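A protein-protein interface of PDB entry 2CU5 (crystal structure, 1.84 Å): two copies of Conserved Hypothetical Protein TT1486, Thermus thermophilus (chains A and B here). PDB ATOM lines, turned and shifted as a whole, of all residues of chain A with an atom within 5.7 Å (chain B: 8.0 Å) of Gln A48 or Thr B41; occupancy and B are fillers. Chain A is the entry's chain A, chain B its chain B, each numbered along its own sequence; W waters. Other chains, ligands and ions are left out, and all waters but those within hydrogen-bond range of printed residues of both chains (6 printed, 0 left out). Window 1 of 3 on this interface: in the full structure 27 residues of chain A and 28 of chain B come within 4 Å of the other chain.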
ATOM      1  N   THR A  46       2.089  17.202  -6.290  1.00  0.00           N
ATOM      2  CA  THR A  46       1.065  16.795  -5.349  1.00  0.00           C
ATOM      3  C   THR A  46       1.702  16.203  -4.106  1.00  0.00           C
ATOM      4  O   THR A  46       2.869  15.791  -4.119  1.00  0.00           O
ATOM      5  CB  THR A  46       0.121  15.726  -5.978  1.00  0.00           C
ATOM      6  OG1 THR A  46      -0.957  15.440  -5.080  1.00  0.00           O
ATOM      7  CG2 THR A  46       0.879  14.439  -6.253  1.00  0.00           C
ATOM      8  N   VAL A  47       0.935  16.194  -3.024  1.00  0.00           N
ATOM      9  CA  VAL A  47       1.384  15.596  -1.778  1.00  0.00           C
ATOM     10  C   VAL A  47       0.471  14.389  -1.589  1.00  0.00           C
ATOM     11  O   VAL A  47      -0.744  14.538  -1.467  1.00  0.00           O
ATOM     12  CB  VAL A  47       1.210  16.546  -0.575  1.00  0.00           C
ATOM     13  CG1 VAL A  47       1.559  15.805   0.704  1.00  0.00           C
ATOM     14  CG2 VAL A  47       2.108  17.778  -0.734  1.00  0.00           C
ATOM     15  N   GLN A  48       1.050  13.195  -1.583  1.00  0.00           N
ATOM     16  CA  GLN A  48       0.263  11.982  -1.429  1.00  0.00           C
ATOM     17  C   GLN A  48       1.018  10.876  -0.710  1.00  0.00           C
ATOM     18  O   GLN A  48       2.117  11.090  -0.202  1.00  0.00           O
ATOM     19  CB  GLN A  48      -0.219  11.494  -2.799  1.00  0.00           C
ATOM     20  CG  GLN A  48      -1.661  11.878  -3.104  1.00  0.00           C
ATOM     21  CD  GLN A  48      -2.621  11.296  -2.085  1.00  0.00           C
ATOM     22  OE1 GLN A  48      -2.511  10.126  -1.718  1.00  0.00           O
ATOM     23  NE2 GLN A  48      -3.570  12.102  -1.630  1.00  0.00           N
ATOM     24  N   GLU A  49       0.427   9.687  -0.666  1.00  0.00           N
ATOM     25  CA  GLU A  49       1.049   8.568   0.025  1.00  0.00           C
ATOM     26  C   GLU A  49       1.970   7.728  -0.852  1.00  0.00           C
ATOM     27  O   GLU A  49       1.605   7.335  -1.962  1.00  0.00           O
ATOM     28  CB  GLU A  49      -0.023   7.658   0.628  1.00  0.00           C
ATOM     29  CG  GLU A  49       0.548   6.661   1.619  1.00  0.00           C
ATOM     30  CD  GLU A  49      -0.428   5.577   2.008  1.00  0.00           C
ATOM     31  OE1 GLU A  49      -1.620   5.880   2.229  1.00  0.00           O
ATOM     32  OE2 GLU A  49       0.010   4.416   2.106  1.00  0.00           O
ATOM     33  N   GLY A  50       3.164   7.452  -0.338  1.00  0.00           N
ATOM     34  CA  GLY A  50       4.114   6.637  -1.069  1.00  0.00           C
ATOM     35  C   GLY A  50       4.374   5.312  -0.372  1.00  0.00           C
ATOM     36  O   GLY A  50       4.808   4.348  -1.005  1.00  0.00           O
ATOM     37  N   VAL A  55      -1.207   2.947  -3.940  1.00  0.00           N
ATOM     38  CA  VAL A  55      -1.914   4.223  -3.907  1.00  0.00           C
ATOM     39  C   VAL A  55      -1.588   4.987  -5.194  1.00  0.00           C
ATOM     40  O   VAL A  55      -2.488   5.463  -5.893  1.00  0.00           O
ATOM     41  CB  VAL A  55      -1.513   5.069  -2.660  1.00  0.00           C
ATOM     42  CG1 VAL A  55      -1.994   6.506  -2.815  1.00  0.00           C
ATOM     43  CG2 VAL A  55      -2.135   4.470  -1.405  1.00  0.00           C
ATOM     44  N   LEU A  59      -4.074   5.889  -8.368  1.00  0.00           N
ATOM     45  CA  LEU A  59      -4.243   7.287  -8.754  1.00  0.00           C
ATOM     46  C   LEU A  59      -4.040   7.466 -10.255  1.00  0.00           C
ATOM     47  O   LEU A  59      -4.845   8.115 -10.929  1.00  0.00           O
ATOM     48  CB  LEU A  59      -3.257   8.188  -7.993  1.00  0.00           C
ATOM     49  CG  LEU A  59      -3.564   8.446  -6.515  1.00  0.00           C
ATOM     50  CD1 LEU A  59      -2.405   9.215  -5.864  1.00  0.00           C
ATOM     51  CD2 LEU A  59      -4.865   9.228  -6.401  1.00  0.00           C
ATOM     52  N   TRP A 108       1.889   9.819   6.503  1.00  0.00           N
ATOM     53  CA  TRP A 108       1.808   9.095   5.233  1.00  0.00           C
ATOM     54  C   TRP A 108       1.931   9.985   4.007  1.00  0.00           C
ATOM     55  O   TRP A 108       1.435   9.633   2.935  1.00  0.00           O
ATOM     56  CB  TRP A 108       0.492   8.323   5.151  1.00  0.00           C
ATOM     57  CG  TRP A 108       0.272   7.420   6.313  1.00  0.00           C
ATOM     58  CD1 TRP A 108      -0.500   7.669   7.411  1.00  0.00           C
ATOM     59  CD2 TRP A 108       0.864   6.134   6.519  1.00  0.00           C
ATOM     60  NE1 TRP A 108      -0.425   6.615   8.291  1.00  0.00           N
ATOM     61  CE2 TRP A 108       0.405   5.659   7.768  1.00  0.00           C
ATOM     62  CE3 TRP A 108       1.737   5.336   5.770  1.00  0.00           C
ATOM     63  CZ2 TRP A 108       0.794   4.417   8.287  1.00  0.00           C
ATOM     64  CZ3 TRP A 108       2.123   4.098   6.287  1.00  0.00           C
ATOM     65  CH2 TRP A 108       1.649   3.654   7.535  1.00  0.00           C
ATOM     66  N   GLN A 109       2.597  11.127   4.156  1.00  0.00           N
ATOM     67  CA  GLN A 109       2.754  12.058   3.043  1.00  0.00           C
ATOM     68  C   GLN A 109       4.168  12.161   2.493  1.00  0.00           C
ATOM     69  O   GLN A 109       5.147  12.090   3.234  1.00  0.00           O
ATOM     70  CB  GLN A 109       2.310  13.467   3.449  1.00  0.00           C
ATOM     71  CG  GLN A 109       0.831  13.644   3.744  1.00  0.00           C
ATOM     72  CD  GLN A 109       0.522  15.077   4.136  1.00  0.00           C
ATOM     73  OE1 GLN A 109       1.197  15.648   4.993  1.00  0.00           O
ATOM     74  NE2 GLN A 109      -0.495  15.668   3.511  1.00  0.00           N
ATOM     75  N   GLN A 110       4.249  12.336   1.178  1.00  0.00           N
ATOM     76  CA  GLN A 110       5.504  12.503   0.459  1.00  0.00           C
ATOM     77  C   GLN A 110       5.218  13.493  -0.672  1.00  0.00           C
ATOM     78  O   GLN A 110       4.080  13.592  -1.142  1.00  0.00           O
ATOM     79  CB  GLN A 110       5.987  11.167  -0.120  1.00  0.00           C
ATOM     80  CG  GLN A 110       6.502  10.184   0.919  1.00  0.00           C
ATOM     81  CD  GLN A 110       7.855  10.581   1.487  1.00  0.00           C
ATOM     82  OE1 GLN A 110       8.892  10.336   0.874  1.00  0.00           O
ATOM     83  NE2 GLN A 110       7.848  11.213   2.658  1.00  0.00           N
ATOM     84  N   VAL A 111       6.235  14.237  -1.096  1.00  0.00           N
ATOM     85  CA  VAL A 111       6.061  15.202  -2.176  1.00  0.00           C
ATOM     86  C   VAL A 111       6.378  14.526  -3.502  1.00  0.00           C
ATOM     87  O   VAL A 111       7.458  13.957  -3.673  1.00  0.00           O
ATOM     88  CB  VAL A 111       6.983  16.427  -1.985  1.00  0.00           C
ATOM     89  CG1 VAL A 111       6.750  17.437  -3.095  1.00  0.00           C
ATOM     90  CG2 VAL A 111       6.716  17.054  -0.634  1.00  0.00           C
ATOM     91  N   PHE A 112       5.433  14.585  -4.438  1.00  0.00           N
ATOM     92  CA  PHE A 112       5.601  13.946  -5.737  1.00  0.00           C
ATOM     93  C   PHE A 112       5.534  14.859  -6.943  1.00  0.00           C
ATOM     94  O   PHE A 112       4.760  15.817  -6.982  1.00  0.00           O
ATOM     95  CB  PHE A 112       4.528  12.873  -5.951  1.00  0.00           C
ATOM     96  CG  PHE A 112       4.664  11.678  -5.067  1.00  0.00           C
ATOM     97  CD1 PHE A 112       5.611  10.695  -5.341  1.00  0.00           C
ATOM     98  CD2 PHE A 112       3.829  11.519  -3.968  1.00  0.00           C
ATOM     99  CE1 PHE A 112       5.722   9.562  -4.528  1.00  0.00           C
ATOM    100  CE2 PHE A 112       3.930  10.402  -3.153  1.00  0.00           C
ATOM    101  CZ  PHE A 112       4.880   9.417  -3.433  1.00  0.00           C
ATOM    102  N   VAL B  38      -3.444  20.308   5.498  1.00  0.00           N
ATOM    103  CA  VAL B  38      -3.930  19.104   6.163  1.00  0.00           C
ATOM    104  C   VAL B  38      -2.867  18.042   5.957  1.00  0.00           C
ATOM    105  O   VAL B  38      -2.512  17.724   4.823  1.00  0.00           O
ATOM    106  CB  VAL B  38      -5.287  18.597   5.595  1.00  0.00           C
ATOM    107  CG1 VAL B  38      -6.401  19.500   6.068  1.00  0.00           C
ATOM    108  CG2 VAL B  38      -5.248  18.533   4.074  1.00  0.00           C
ATOM    109  N   PRO B  39      -2.320  17.501   7.056  1.00  0.00           N
ATOM    110  CA  PRO B  39      -1.282  16.470   6.993  1.00  0.00           C
ATOM    111  C   PRO B  39      -1.912  15.103   6.757  1.00  0.00           C
ATOM    112  O   PRO B  39      -1.596  14.134   7.447  1.00  0.00           O
ATOM    113  CB  PRO B  39      -0.623  16.574   8.367  1.00  0.00           C
ATOM    114  CG  PRO B  39      -1.786  16.883   9.251  1.00  0.00           C
ATOM    115  CD  PRO B  39      -2.573  17.911   8.453  1.00  0.00           C
ATOM    116  N   HIS B  40      -2.800  15.039   5.771  1.00  0.00           N
ATOM    117  CA  HIS B  40      -3.517  13.807   5.471  1.00  0.00           C
ATOM    118  C   HIS B  40      -3.586  13.584   3.972  1.00  0.00           C
ATOM    119  O   HIS B  40      -3.471  14.528   3.199  1.00  0.00           O
ATOM    120  CB  HIS B  40      -4.935  13.898   6.032  1.00  0.00           C
ATOM    121  CG  HIS B  40      -4.989  14.285   7.475  1.00  0.00           C
ATOM    122  ND1 HIS B  40      -4.548  13.458   8.484  1.00  0.00           N
ATOM    123  CD2 HIS B  40      -5.431  15.413   8.078  1.00  0.00           C
ATOM    124  CE1 HIS B  40      -4.719  14.059   9.648  1.00  0.00           C
ATOM    125  NE2 HIS B  40      -5.255  15.246   9.429  1.00  0.00           N
ATOM    126  N   THR B  41      -3.802  12.338   3.565  1.00  0.00           N
ATOM    127  CA  THR B  41      -3.860  12.013   2.147  1.00  0.00           C
ATOM    128  C   THR B  41      -5.245  11.594   1.656  1.00  0.00           C
ATOM    129  O   THR B  41      -5.406  11.300   0.473  1.00  0.00           O
ATOM    130  CB  THR B  41      -2.880  10.872   1.799  1.00  0.00           C
ATOM    131  OG1 THR B  41      -3.215   9.712   2.568  1.00  0.00           O
ATOM    132  CG2 THR B  41      -1.434  11.282   2.104  1.00  0.00           C
ATOM    133  N   THR B  42      -6.232  11.542   2.550  1.00  0.00           N
ATOM    134  CA  THR B  42      -7.578  11.152   2.140  1.00  0.00           C
ATOM    135  C   THR B  42      -8.644  12.201   2.442  1.00  0.00           C
ATOM    136  O   THR B  42      -9.836  11.897   2.525  1.00  0.00           O
ATOM    137  CB  THR B  42      -7.994   9.779   2.739  1.00  0.00           C
ATOM    138  OG1 THR B  42      -7.894   9.808   4.167  1.00  0.00           O
ATOM    139  CG2 THR B  42      -7.097   8.678   2.187  1.00  0.00           C
ATOM    140  N   CYS B  43      -8.200  13.441   2.620  1.00  0.00           N
ATOM    141  CA  CYS B  43      -9.110  14.559   2.832  1.00  0.00           C
ATOM    142  C   CYS B  43      -8.414  15.745   2.182  1.00  0.00           C
ATOM    143  O   CYS B  43      -7.252  15.630   1.773  1.00  0.00           O
ATOM    144  CB  CYS B  43      -9.380  14.807   4.328  1.00  0.00           C
ATOM    145  SG  CYS B  43      -8.003  15.437   5.315  1.00  0.00           S
ATOM    146  N   GLY B  44      -9.111  16.864   2.045  1.00  0.00           N
ATOM    147  CA  GLY B  44      -8.494  18.018   1.421  1.00  0.00           C
ATOM    148  C   GLY B  44      -8.972  19.353   1.954  1.00  0.00           C
ATOM    149  O   GLY B  44      -9.762  19.415   2.901  1.00  0.00           O
ATOM    150  N   HIS B  76      -5.094  -0.991  -4.377  1.00  0.00           N
ATOM    151  CA  HIS B  76      -4.993  -0.555  -2.984  1.00  0.00           C
ATOM    152  C   HIS B  76      -6.134  -1.245  -2.239  1.00  0.00           C
ATOM    153  O   HIS B  76      -7.258  -0.741  -2.190  1.00  0.00           O
ATOM    154  CB  HIS B  76      -5.136   0.967  -2.911  1.00  0.00           C
ATOM    155  CG  HIS B  76      -4.924   1.538  -1.543  1.00  0.00           C
ATOM    156  ND1 HIS B  76      -3.793   1.287  -0.797  1.00  0.00           N
ATOM    157  CD2 HIS B  76      -5.683   2.381  -0.805  1.00  0.00           C
ATOM    158  CE1 HIS B  76      -3.863   1.953   0.342  1.00  0.00           C
ATOM    159  NE2 HIS B  76      -5.000   2.626   0.361  1.00  0.00           N
ATOM    160  N   ASN B  80      -9.539   2.742  -0.026  1.00  0.00           N
ATOM    161  CA  ASN B  80      -9.810   4.171  -0.010  1.00  0.00           C
ATOM    162  C   ASN B  80      -9.108   4.952  -1.112  1.00  0.00           C
ATOM    163  O   ASN B  80      -8.885   6.151  -0.986  1.00  0.00           O
ATOM    164  CB  ASN B  80      -9.485   4.771   1.370  1.00  0.00           C
ATOM    165  CG  ASN B  80      -8.023   4.656   1.729  1.00  0.00           C
ATOM    166  OD1 ASN B  80      -7.232   4.075   0.988  1.00  0.00           O
ATOM    167  ND2 ASN B  80      -7.653   5.213   2.878  1.00  0.00           N
ATOM    168  N   SER B  81      -8.778   4.292  -2.214  1.00  0.00           N
ATOM    169  CA  SER B  81      -8.125   5.007  -3.303  1.00  0.00           C
ATOM    170  C   SER B  81      -9.031   6.124  -3.818  1.00  0.00           C
ATOM    171  O   SER B  81      -8.548   7.140  -4.316  1.00  0.00           O
ATOM    172  CB  SER B  81      -7.772   4.062  -4.445  1.00  0.00           C
ATOM    173  OG  SER B  81      -6.657   3.273  -4.101  1.00  0.00           O
ATOM    174  N   HIS B  82     -10.344   5.938  -3.701  1.00  0.00           N
ATOM    175  CA  HIS B  82     -11.272   6.966  -4.157  1.00  0.00           C
ATOM    176  C   HIS B  82     -11.014   8.245  -3.368  1.00  0.00           C
ATOM    177  O   HIS B  82     -11.089   9.346  -3.914  1.00  0.00           O
ATOM    178  CB  HIS B  82     -12.732   6.526  -3.958  1.00  0.00           C
ATOM    179  CG  HIS B  82     -13.191   6.537  -2.531  1.00  0.00           C
ATOM    180  ND1 HIS B  82     -12.737   5.636  -1.589  1.00  0.00           N
ATOM    181  CD2 HIS B  82     -14.075   7.336  -1.888  1.00  0.00           C
ATOM    182  CE1 HIS B  82     -13.323   5.879  -0.431  1.00  0.00           C
ATOM    183  NE2 HIS B  82     -14.140   6.906  -0.584  1.00  0.00           N
ATOM    184  N   ALA B  83     -10.711   8.082  -2.084  1.00  0.00           N
ATOM    185  CA  ALA B  83     -10.450   9.218  -1.198  1.00  0.00           C
ATOM    186  C   ALA B  83      -9.101   9.854  -1.520  1.00  0.00           C
ATOM    187  O   ALA B  83      -8.954  11.071  -1.446  1.00  0.00           O
ATOM    188  CB  ALA B  83     -10.492   8.767   0.264  1.00  0.00           C
ATOM    189  N   HIS B  84      -8.118   9.028  -1.863  1.00  0.00           N
ATOM    190  CA  HIS B  84      -6.801   9.543  -2.223  1.00  0.00           C
ATOM    191  C   HIS B  84      -6.947  10.400  -3.482  1.00  0.00           C
ATOM    192  O   HIS B  84      -6.354  11.476  -3.588  1.00  0.00           O
ATOM    193  CB  HIS B  84      -5.830   8.387  -2.480  1.00  0.00           C
ATOM    194  CG  HIS B  84      -5.274   7.777  -1.232  1.00  0.00           C
ATOM    195  ND1 HIS B  84      -4.211   8.326  -0.547  1.00  0.00           N
ATOM    196  CD2 HIS B  84      -5.648   6.682  -0.530  1.00  0.00           C
ATOM    197  CE1 HIS B  84      -3.952   7.594   0.522  1.00  0.00           C
ATOM    198  NE2 HIS B  84      -4.809   6.591   0.556  1.00  0.00           N
ATOM    199  N   LEU B  85      -7.751   9.929  -4.432  1.00  0.00           N
ATOM    200  CA  LEU B  85      -7.958  10.678  -5.668  1.00  0.00           C
ATOM    201  C   LEU B  85      -8.670  11.993  -5.408  1.00  0.00           C
ATOM    202  O   LEU B  85      -8.265  13.033  -5.925  1.00  0.00           O
ATOM    203  CB  LEU B  85      -8.763   9.859  -6.681  1.00  0.00           C
ATOM    204  CG  LEU B  85      -9.117  10.602  -7.979  1.00  0.00           C
ATOM    205  CD1 LEU B  85      -7.851  11.097  -8.676  1.00  0.00           C
ATOM    206  CD2 LEU B  85      -9.884   9.654  -8.907  1.00  0.00           C
ATOM    207  N   LYS B  86      -9.739  11.954  -4.616  1.00  0.00           N
ATOM    208  CA  LYS B  86     -10.474  13.178  -4.308  1.00  0.00           C
ATOM    209  C   LYS B  86      -9.550  14.174  -3.610  1.00  0.00           C
ATOM    210  O   LYS B  86      -9.628  15.380  -3.850  1.00  0.00           O
ATOM    211  CB  LYS B  86     -11.684  12.867  -3.426  1.00  0.00           C
ATOM    212  CG  LYS B  86     -12.741  12.034  -4.138  1.00  0.00           C
ATOM    213  CD  LYS B  86     -13.825  11.579  -3.193  1.00  0.00           C
ATOM    214  CE  LYS B  86     -14.737  10.560  -3.865  1.00  0.00           C
ATOM    215  NZ  LYS B  86     -15.701   9.977  -2.900  1.00  0.00           N
ATOM    216  N   SER B  87      -8.672  13.666  -2.751  1.00  0.00           N
ATOM    217  CA  SER B  87      -7.723  14.535  -2.051  1.00  0.00           C
ATOM    218  C   SER B  87      -6.785  15.220  -3.057  1.00  0.00           C
ATOM    219  O   SER B  87      -6.584  16.434  -3.000  1.00  0.00           O
ATOM    220  CB  SER B  87      -6.900  13.720  -1.050  1.00  0.00           C
ATOM    221  OG  SER B  87      -5.952  14.540  -0.384  1.00  0.00           O
ATOM    222  N   LEU B  88      -6.219  14.439  -3.974  1.00  0.00           N
ATOM    223  CA  LEU B  88      -5.312  14.971  -4.995  1.00  0.00           C
ATOM    224  C   LEU B  88      -5.996  16.020  -5.869  1.00  0.00           C
ATOM    225  O   LEU B  88      -5.403  17.046  -6.216  1.00  0.00           O
ATOM    226  CB  LEU B  88      -4.772  13.827  -5.876  1.00  0.00           C
ATOM    227  CG  LEU B  88      -3.865  14.212  -7.059  1.00  0.00           C
ATOM    228  CD1 LEU B  88      -2.956  13.043  -7.417  1.00  0.00           C
ATOM    229  CD2 LEU B  88      -4.716  14.634  -8.265  1.00  0.00           C
ATOM    230  N   LEU B  89      -7.251  15.756  -6.225  1.00  0.00           N
ATOM    231  CA  LEU B  89      -8.020  16.670  -7.062  1.00  0.00           C
ATOM    232  C   LEU B  89      -8.378  17.976  -6.353  1.00  0.00           C
ATOM    233  O   LEU B  89      -8.477  19.026  -6.985  1.00  0.00           O
ATOM    234  CB  LEU B  89      -9.311  15.990  -7.531  1.00  0.00           C
ATOM    235  CG  LEU B  89      -9.154  14.770  -8.441  1.00  0.00           C
ATOM    236  CD1 LEU B  89     -10.520  14.152  -8.700  1.00  0.00           C
ATOM    237  CD2 LEU B  89      -8.496  15.180  -9.745  1.00  0.00           C
ATOM    238  N   GLY B  91      -6.712  19.169  -3.334  1.00  0.00           N
ATOM    239  CA  GLY B  91      -5.500  19.826  -2.874  1.00  0.00           C
ATOM    240  C   GLY B  91      -5.462  19.753  -1.360  1.00  0.00           C
ATOM    241  O   GLY B  91      -6.506  19.574  -0.726  1.00  0.00           O
ATOM    242  N   VAL B  92      -4.279  19.894  -0.768  1.00  0.00           N
ATOM    243  CA  VAL B  92      -4.167  19.804   0.681  1.00  0.00           C
ATOM    244  C   VAL B  92      -3.666  21.064   1.390  1.00  0.00           C
ATOM    245  O   VAL B  92      -3.299  21.011   2.566  1.00  0.00           O
ATOM    246  CB  VAL B  92      -3.272  18.615   1.093  1.00  0.00           C
ATOM    247  CG1 VAL B  92      -3.858  17.317   0.541  1.00  0.00           C
ATOM    248  CG2 VAL B  92      -1.851  18.811   0.569  1.00  0.00           C
ATOM    249  N   GLU B 115     -13.651  16.196   3.755  1.00  0.00           N
ATOM    250  CA  GLU B 115     -13.413  14.840   4.230  1.00  0.00           C
ATOM    251  C   GLU B 115     -13.958  13.821   3.245  1.00  0.00           C
ATOM    252  O   GLU B 115     -15.127  13.882   2.863  1.00  0.00           O
ATOM    253  CB  GLU B 115     -14.078  14.618   5.590  1.00  0.00           C
ATOM    254  CG  GLU B 115     -13.926  13.192   6.094  1.00  0.00           C
ATOM    255  CD  GLU B 115     -12.477  12.817   6.375  1.00  0.00           C
ATOM    256  OE1 GLU B 115     -11.986  13.136   7.479  1.00  0.00           O
ATOM    257  OE2 GLU B 115     -11.822  12.213   5.494  1.00  0.00           O
ATOM    258  N   PHE B 116     -13.111  12.875   2.851  1.00  0.00           N
ATOM    259  CA  PHE B 116     -13.513  11.835   1.904  1.00  0.00           C
ATOM    260  C   PHE B 116     -13.398  10.443   2.494  1.00  0.00           C
ATOM    261  O   PHE B 116     -13.804   9.466   1.866  1.00  0.00           O
ATOM    262  CB  PHE B 116     -12.636  11.902   0.652  1.00  0.00           C
ATOM    263  CG  PHE B 116     -12.642  13.237  -0.021  1.00  0.00           C
ATOM    264  CD1 PHE B 116     -13.838  13.806  -0.456  1.00  0.00           C
ATOM    265  CD2 PHE B 116     -11.450  13.935  -0.229  1.00  0.00           C
ATOM    266  CE1 PHE B 116     -13.854  15.041  -1.087  1.00  0.00           C
ATOM    267  CE2 PHE B 116     -11.458  15.177  -0.860  1.00  0.00           C
ATOM    268  CZ  PHE B 116     -12.660  15.732  -1.292  1.00  0.00           C
ATOM    269  N   ASP B 117     -12.865  10.348   3.708  1.00  0.00           N
ATOM    270  CA  ASP B 117     -12.647   9.046   4.329  1.00  0.00           C
ATOM    271  C   ASP B 117     -12.734   9.096   5.859  1.00  0.00           C
ATOM    272  O   ASP B 117     -11.794   8.714   6.560  1.00  0.00           O
ATOM    273  CB  ASP B 117     -11.268   8.539   3.869  1.00  0.00           C
ATOM    274  CG  ASP B 117     -10.989   7.098   4.264  1.00  0.00           C
ATOM    275  OD1 ASP B 117     -11.924   6.271   4.298  1.00  0.00           O
ATOM    276  OD2 ASP B 117      -9.805   6.789   4.515  1.00  0.00           O
ATOM    277  N   ARG B 120     -13.683  10.925  11.528  1.00  0.00           N
ATOM    278  CA  ARG B 120     -12.482  10.952  12.354  1.00  0.00           C
ATOM    279  C   ARG B 120     -12.155  12.390  12.713  1.00  0.00           C
ATOM    280  O   ARG B 120     -12.929  13.295  12.430  1.00  0.00           O
ATOM    281  CB  ARG B 120     -11.320  10.343  11.564  1.00  0.00           C
ATOM    282  CG  ARG B 120     -11.064  11.050  10.238  1.00  0.00           C
ATOM    283  CD  ARG B 120     -10.534  10.101   9.164  1.00  0.00           C
ATOM    284  NE  ARG B 120      -9.164   9.657   9.415  1.00  0.00           N
ATOM    285  CZ  ARG B 120      -8.469   8.882   8.583  1.00  0.00           C
ATOM    286  NH1 ARG B 120      -7.227   8.523   8.882  1.00  0.00           N
ATOM    287  NH2 ARG B 120      -9.018   8.459   7.450  1.00  0.00           N
ATOM    288  N   ARG B 122      -9.428  15.326  12.084  1.00  0.00           N
ATOM    289  CA  ARG B 122      -8.338  15.713  11.209  1.00  0.00           C
ATOM    290  C   ARG B 122      -7.655  16.928  11.803  1.00  0.00           C
ATOM    291  O   ARG B 122      -8.271  17.702  12.535  1.00  0.00           O
ATOM    292  CB  ARG B 122      -8.865  16.102   9.829  1.00  0.00           C
ATOM    293  CG  ARG B 122      -9.631  15.020   9.109  1.00  0.00           C
ATOM    294  CD  ARG B 122      -8.741  13.845   8.788  1.00  0.00           C
ATOM    295  NE  ARG B 122      -9.294  13.085   7.668  1.00  0.00           N
ATOM    296  CZ  ARG B 122      -8.652  12.105   7.043  1.00  0.00           C
ATOM    297  NH1 ARG B 122      -9.236  11.476   6.034  1.00  0.00           N
ATOM    298  NH2 ARG B 122      -7.433  11.752   7.427  1.00  0.00           N
HETATM  299  O   HOH W   1      -4.975   5.836  -4.395  1.00  0.00           O
HETATM  300  O   HOH W   2      -3.500  14.995  -2.226  1.00  0.00           O
HETATM  301  O   HOH W   3      -4.366   4.724   2.575  1.00  0.00           O
HETATM  302  O   HOH W   4      -0.378  11.482   6.299  1.00  0.00           O
HETATM  303  O   HOH W   5      -1.600  14.446   1.277  1.00  0.00           O
HETATM  304  O   HOH W   6      -2.782  17.556  -5.590  1.00  0.00           O
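Printed residues of chain B within 4 Å of Gln A48: Thr B41 (2.9 Å), His B84 (2.7 Å) and Ser B87 (3.6 Å). Thr B41 touches just these residues of chain A: Gln A48, Glu A49, Trp A108 and Gln A109. Of the printed residues of chain A, His B40 touches Gln A109. Of the printed residues of chain B, Thr A46 touches Leu B88. Of the printed residues of chain A, Leu B85 touches Leu A59. Printed residues of chain A within 4 Å of Ser B87: Gln A48 (3.6 Å). Printed residues of chain A within 4 Å of Pro B39: Gln A109. Cys B43 touches none of the printed residues of chain A. The nearest residue of chain B that does not touch Gln A48 is Leu B88 (4.2 Å). The nearest printed residue of chain B that does not touch Glu A49 is His B76 (4.9 Å).
A ring nitrogen (NE2) of His B76 sits at hydrogen-bond distance from the side-chain amide oxygen of Asn B80, at 2.7 Å. The backbone NH (N) of Gln A110 sits at hydrogen-bond distance from the backbone carbonyl oxygen (O) of Gln A48, at 2.8 Å. O of Cys B43 is in hydrogen-bond range of OG of Ser B87 (2.7 Å). The backbone carbonyl oxygen (O) of Thr A46 lies within hydrogen-bond range of the backbone NH (N) of Phe A112 (2.9 Å). The backbone carbonyl oxygen (O) of Thr B41 lies close to the side-chain hydroxyl (OG) of Ser B87, 3.4 Å away. The backbone carbonyl oxygen (O) of Val B92 sits at hydrogen-bond distance from the backbone NH (N) of Val B38 (3.0 Å).
Water W5 lies within hydrogen-bond range of the backbone carbonyl oxygen (O) of His B40, the side-chain amide nitrogen (NE2) of Gln A109 and the backbone carbonyl oxygen (O) of Val A47. Water W6 bridges the backbone carbonyl oxygen of Leu B88 and the side-chain hydroxyl of Thr A46. Water W3 lies within hydrogen-bond range of a ring nitrogen (NE2) of His B84, the side-chain carboxylate of Glu A49, a ring nitrogen (NE2) of His B76 and the side-chain amide nitrogen of Asn B80. Water W1 lies within hydrogen-bond range of O of Val A55 (2.9 Å) and OG of Ser B81 (3.1 Å).
Among the printed residues, pairs that only touch across the chains: Thr A46 with Leu B88 (3.7 Å), Val A47 with Val B92 (3.98 Å), Gln A48 with Ser B87 (3.6 Å), Glu A49 with Thr B41 (3.7 Å), Glu A49 with His B84 (3.4 Å), Val A55 with His B76 (3.5 Å), Val A55 with His B84 (3.7 Å), Leu A59 with His B84 (3.8 Å), Leu A59 with Leu B85 (3.5 Å), Trp A108 with Thr B41 (3.4 Å), Gln A109 with Pro B39 (3.3 Å) and Gln A109 with Thr B41 (3.7 Å).
The backbone carbonyl oxygen (O) of Thr B41 sits at hydrogen-bond distance from the side-chain amide nitrogen (NE2) of Gln A48 (2.9 Å). OE1 of Gln A48 lies within hydrogen-bond range of ND1 of His B84 (2.7 Å). The backbone carbonyl oxygen of Val B38 sits at hydrogen-bond distance from the side-chain amide nitrogen of Gln A109, 3.2 Å away. NE2 of Gln A109 is in hydrogen-bond range of O of His B40 (3.2 Å).
No position is printed for both chains. Of the 16 pairs that touch across the chains among the printed residues, none has its exchanged pair printed and touching as well.
Hydrophobic or aromatic side chains of chain A within 4 Å of the printed part of chain B: Val A47, Val A55 and Leu A59. Of the 25 printed residues of chain B, 10 touch a printed residue of chain A. Hydrophobic or aromatic side chains of chain B that line the printed part of chain A: Pro B39, His B76, His B84, Leu B85, Leu B88 and Val B92. Among the printed residues, 16 pairs touch across the chains.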
